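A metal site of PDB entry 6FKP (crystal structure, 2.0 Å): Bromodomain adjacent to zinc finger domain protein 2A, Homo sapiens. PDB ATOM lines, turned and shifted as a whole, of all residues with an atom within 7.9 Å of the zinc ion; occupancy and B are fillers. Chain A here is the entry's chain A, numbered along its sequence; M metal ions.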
ATOM      1  N   THR A   8       0.790   4.188  22.052  1.00  0.00           N
ATOM      2  CA  THR A   8       1.742   5.287  22.100  1.00  0.00           C
ATOM      3  C   THR A   8       0.994   6.609  22.033  1.00  0.00           C
ATOM      4  O   THR A   8      -0.138   6.686  21.557  1.00  0.00           O
ATOM      5  CB  THR A   8       2.763   5.205  20.946  1.00  0.00           C
ATOM      6  OG1 THR A   8       2.075   5.215  19.692  1.00  0.00           O
ATOM      7  CG2 THR A   8       3.611   3.946  21.062  1.00  0.00           C
ATOM      8  N   CYS A   9       1.658   7.653  22.507  1.00  0.00           N
ATOM      9  CA  CYS A   9       1.089   8.995  22.556  1.00  0.00           C
ATOM     10  C   CYS A   9       1.130   9.636  21.163  1.00  0.00           C
ATOM     11  O   CYS A   9       2.151   9.578  20.481  1.00  0.00           O
ATOM     12  CB  CYS A   9       1.847   9.821  23.586  1.00  0.00           C
ATOM     13  SG  CYS A   9       1.632  11.613  23.552  1.00  0.00           S
ATOM     14  N   LEU A  10       0.015  10.249  20.766  1.00  0.00           N
ATOM     15  CA  LEU A  10      -0.081  10.925  19.458  1.00  0.00           C
ATOM     16  C   LEU A  10       0.894  12.088  19.271  1.00  0.00           C
ATOM     17  O   LEU A  10       1.292  12.382  18.141  1.00  0.00           O
ATOM     18  CB  LEU A  10      -1.501  11.456  19.233  1.00  0.00           C
ATOM     19  CG  LEU A  10      -2.576  10.448  18.856  1.00  0.00           C
ATOM     20  CD1 LEU A  10      -3.956  11.070  19.041  1.00  0.00           C
ATOM     21  CD2 LEU A  10      -2.383   9.977  17.427  1.00  0.00           C
ATOM     22  N   VAL A  11       1.249  12.769  20.351  1.00  0.00           N
ATOM     23  CA  VAL A  11       2.108  13.953  20.288  1.00  0.00           C
ATOM     24  C   VAL A  11       3.594  13.570  20.217  1.00  0.00           C
ATOM     25  O   VAL A  11       4.264  13.913  19.249  1.00  0.00           O
ATOM     26  CB  VAL A  11       1.859  14.895  21.498  1.00  0.00           C
ATOM     27  CG1 VAL A  11       2.785  16.109  21.463  1.00  0.00           C
ATOM     28  CG2 VAL A  11       0.396  15.317  21.534  1.00  0.00           C
ATOM     29  N   CYS A  12       4.087  12.859  21.228  1.00  0.00           N
ATOM     30  CA  CYS A  12       5.519  12.550  21.342  1.00  0.00           C
ATOM     31  C   CYS A  12       5.932  11.176  20.773  1.00  0.00           C
ATOM     32  O   CYS A  12       7.121  10.876  20.726  1.00  0.00           O
ATOM     33  CB  CYS A  12       5.959  12.657  22.791  1.00  0.00           C
ATOM     34  SG  CYS A  12       5.354  11.339  23.870  1.00  0.00           S
ATOM     35  N   ARG A  13       4.956  10.363  20.367  1.00  0.00           N
ATOM     36  CA  ARG A  13       5.198   9.023  19.781  1.00  0.00           C
ATOM     37  C   ARG A  13       5.844   7.993  20.719  1.00  0.00           C
ATOM     38  O   ARG A  13       6.423   7.018  20.251  1.00  0.00           O
ATOM     39  CB  ARG A  13       6.016   9.137  18.470  1.00  0.00           C
ATOM     40  CG  ARG A  13       5.483  10.136  17.451  1.00  0.00           C
ATOM     41  CD  ARG A  13       4.139   9.673  16.900  1.00  0.00           C
ATOM     42  NE  ARG A  13       3.735  10.466  15.739  1.00  0.00           N
ATOM     43  N   LYS A  14       5.726   8.189  22.044  1.00  0.00           N
ATOM     44  CA  LYS A  14       6.286   7.241  23.021  1.00  0.00           C
ATOM     45  C   LYS A  14       5.189   6.645  23.900  1.00  0.00           C
ATOM     46  O   LYS A  14       4.140   7.268  24.108  1.00  0.00           O
ATOM     47  CB  LYS A  14       7.365   7.890  23.886  1.00  0.00           C
ATOM     48  CG  LYS A  14       8.461   8.586  23.085  1.00  0.00           C
ATOM     49  CD  LYS A  14       9.655   8.991  23.929  1.00  0.00           C
ATOM     50  CE  LYS A  14       9.371  10.217  24.769  1.00  0.00           C
ATOM     51  NZ  LYS A  14      10.623  10.759  25.396  1.00  0.00           N
ATOM     52  N   GLY A  15       5.432   5.437  24.386  1.00  0.00           N
ATOM     53  CA  GLY A  15       4.498   4.716  25.257  1.00  0.00           C
ATOM     54  C   GLY A  15       4.916   4.650  26.710  1.00  0.00           C
ATOM     55  O   GLY A  15       4.345   3.874  27.476  1.00  0.00           O
ATOM     56  N   ASP A  16       5.903   5.462  27.106  1.00  0.00           N
ATOM     57  CA  ASP A  16       6.375   5.506  28.505  1.00  0.00           C
ATOM     58  C   ASP A  16       5.382   6.220  29.431  1.00  0.00           C
ATOM     59  O   ASP A  16       4.436   6.854  28.964  1.00  0.00           O
ATOM     60  CB  ASP A  16       7.778   6.138  28.598  1.00  0.00           C
ATOM     61  CG  ASP A  16       7.832   7.585  28.077  1.00  0.00           C
ATOM     62  OD1 ASP A  16       6.893   8.018  27.381  1.00  0.00           O
ATOM     63  OD2 ASP A  16       8.837   8.272  28.353  1.00  0.00           O
ATOM     64  N   PHE A  20       0.206   8.231  33.036  1.00  0.00           N
ATOM     65  CA  PHE A  20      -0.186   9.533  32.472  1.00  0.00           C
ATOM     66  C   PHE A  20      -0.729   9.437  31.035  1.00  0.00           C
ATOM     67  O   PHE A  20      -1.161  10.452  30.463  1.00  0.00           O
ATOM     68  CB  PHE A  20       1.014  10.484  32.495  1.00  0.00           C
ATOM     69  CG  PHE A  20       1.452  10.858  33.884  1.00  0.00           C
ATOM     70  CD1 PHE A  20       2.280  10.008  34.610  1.00  0.00           C
ATOM     71  CD2 PHE A  20       1.049  12.058  34.451  1.00  0.00           C
ATOM     72  CE1 PHE A  20       2.686  10.351  35.893  1.00  0.00           C
ATOM     73  CE2 PHE A  20       1.464  12.405  35.732  1.00  0.00           C
ATOM     74  CZ  PHE A  20       2.272  11.548  36.447  1.00  0.00           C
ATOM     75  N   LEU A  21      -0.750   8.227  30.459  1.00  0.00           N
ATOM     76  CA  LEU A  21      -1.029   8.010  29.041  1.00  0.00           C
ATOM     77  C   LEU A  21      -2.519   7.747  28.829  1.00  0.00           C
ATOM     78  O   LEU A  21      -2.968   6.606  28.900  1.00  0.00           O
ATOM     79  CB  LEU A  21      -0.186   6.843  28.518  1.00  0.00           C
ATOM     80  CG  LEU A  21      -0.328   6.446  27.040  1.00  0.00           C
ATOM     81  CD1 LEU A  21      -0.156   7.640  26.112  1.00  0.00           C
ATOM     82  CD2 LEU A  21       0.687   5.361  26.700  1.00  0.00           C
ATOM     83  N   GLY A  30      -3.803   7.185  21.916  1.00  0.00           N
ATOM     84  CA  GLY A  30      -3.496   7.694  23.250  1.00  0.00           C
ATOM     85  C   GLY A  30      -2.796   9.028  23.240  1.00  0.00           C
ATOM     86  O   GLY A  30      -2.321   9.499  22.199  1.00  0.00           O
ATOM     87  N   CYS A  31      -2.731   9.647  24.421  1.00  0.00           N
ATOM     88  CA  CYS A  31      -2.011  10.907  24.586  1.00  0.00           C
ATOM     89  C   CYS A  31      -1.626  11.096  26.055  1.00  0.00           C
ATOM     90  O   CYS A  31      -2.474  10.937  26.939  1.00  0.00           O
ATOM     91  CB  CYS A  31      -2.875  12.082  24.109  1.00  0.00           C
ATOM     92  SG  CYS A  31      -2.077  13.711  24.148  1.00  0.00           S
ATOM     93  N   HIS A  32      -0.366  11.419  26.306  1.00  0.00           N
ATOM     94  CA  HIS A  32       0.064  11.798  27.654  1.00  0.00           C
ATOM     95  C   HIS A  32      -0.662  13.068  28.054  1.00  0.00           C
ATOM     96  O   HIS A  32      -0.711  14.026  27.272  1.00  0.00           O
ATOM     97  CB  HIS A  32       1.562  12.084  27.730  1.00  0.00           C
ATOM     98  CG  HIS A  32       2.409  10.885  27.499  1.00  0.00           C
ATOM     99  ND1 HIS A  32       3.215  10.752  26.390  1.00  0.00           N
ATOM    100  CD2 HIS A  32       2.591   9.758  28.236  1.00  0.00           C
ATOM    101  CE1 HIS A  32       3.859   9.597  26.459  1.00  0.00           C
ATOM    102  NE2 HIS A  32       3.501   8.975  27.562  1.00  0.00           N
ATOM    103  N   ILE A  33      -1.194  13.105  29.278  1.00  0.00           N
ATOM    104  CA  ILE A  33      -1.826  14.333  29.772  1.00  0.00           C
ATOM    105  C   ILE A  33      -0.856  15.524  29.749  1.00  0.00           C
ATOM    106  O   ILE A  33      -1.279  16.652  29.493  1.00  0.00           O
ATOM    107  CB  ILE A  33      -2.484  14.176  31.166  1.00  0.00           C
ATOM    108  CG1 ILE A  33      -1.455  13.895  32.263  1.00  0.00           C
ATOM    109  CG2 ILE A  33      -3.562  13.091  31.135  1.00  0.00           C
ATOM    110  CD1 ILE A  33      -2.067  13.858  33.657  1.00  0.00           C
ATOM    111  N   TYR A  34       0.429  15.256  29.979  1.00  0.00           N
ATOM    112  CA  TYR A  34       1.448  16.310  29.959  1.00  0.00           C
ATOM    113  C   TYR A  34       1.860  16.778  28.567  1.00  0.00           C
ATOM    114  O   TYR A  34       2.467  17.841  28.430  1.00  0.00           O
ATOM    115  CB  TYR A  34       2.679  15.923  30.798  1.00  0.00           C
ATOM    116  CG  TYR A  34       3.342  14.611  30.440  1.00  0.00           C
ATOM    117  CD1 TYR A  34       4.192  14.504  29.333  1.00  0.00           C
ATOM    118  CD2 TYR A  34       3.151  13.470  31.218  1.00  0.00           C
ATOM    119  CE1 TYR A  34       4.809  13.306  29.012  1.00  0.00           C
ATOM    120  CE2 TYR A  34       3.758  12.273  30.905  1.00  0.00           C
ATOM    121  CZ  TYR A  34       4.596  12.197  29.812  1.00  0.00           C
ATOM    122  OH  TYR A  34       5.212  11.004  29.499  1.00  0.00           O
ATOM    123  N   CYS A  35       1.524  16.013  27.523  1.00  0.00           N
ATOM    124  CA  CYS A  35       1.726  16.434  26.124  1.00  0.00           C
ATOM    125  C   CYS A  35       0.520  17.188  25.566  1.00  0.00           C
ATOM    126  O   CYS A  35       0.652  17.876  24.560  1.00  0.00           O
ATOM    127  CB  CYS A  35       2.011  15.237  25.216  1.00  0.00           C
ATOM    128  SG  CYS A  35       3.557  14.386  25.596  1.00  0.00           S
ATOM    129  N   HIS A  36      -0.633  17.064  26.225  1.00  0.00           N
ATOM    130  CA  HIS A  36      -1.852  17.724  25.765  1.00  0.00           C
ATOM    131  C   HIS A  36      -1.756  19.264  25.849  1.00  0.00           C
ATOM    132  O   HIS A  36      -1.195  19.790  26.802  1.00  0.00           O
ATOM    133  CB  HIS A  36      -3.055  17.230  26.581  1.00  0.00           C
ATOM    134  CG  HIS A  36      -4.370  17.444  25.893  1.00  0.00           C
ATOM    135  ND1 HIS A  36      -4.990  18.676  25.837  1.00  0.00           N
ATOM    136  CD2 HIS A  36      -5.163  16.590  25.206  1.00  0.00           C
ATOM    137  CE1 HIS A  36      -6.120  18.568  25.157  1.00  0.00           C
ATOM    138  NE2 HIS A  36      -6.241  17.306  24.758  1.00  0.00           N
HETATM  139 ZN    ZN M   1       3.434  12.169  24.904  1.00  0.00          ZN
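The zinc ion is bound by a ring nitrogen (ND1) of His 32 (2.1 Å), the side-chain sulfur of Cys 9 (2.3 Å), the side-chain sulfur of Cys 35 (2.3 Å) and the side-chain sulfur of Cys 12 (2.3 Å).
The zinc ion has four donor atoms within binding distance.
NE2 of His 32 sits close to OH of Tyr 34 (3.3 Å).
NE2 of His 32 sits at hydrogen-bond distance from O of Asp 16, 2.7 Å away.
The side-chain sulfur of Cys 9 sits close to the backbone NH of Val 11, at 3.4 Å.
The backbone carbonyl oxygen of Lys 14 lies within hydrogen-bond range of the backbone NH of Cys 9 (3.0 Å).
The side-chain sulfur (SG) of Cys 12 sits close to the backbone NH (N) of Lys 14.
Within 4 Å of the zinc ion: Cys 9, Cys 12, His 32 and Cys 35.
Along chain A the residues within 4 Å of the zinc ion span positions 9 to 35.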
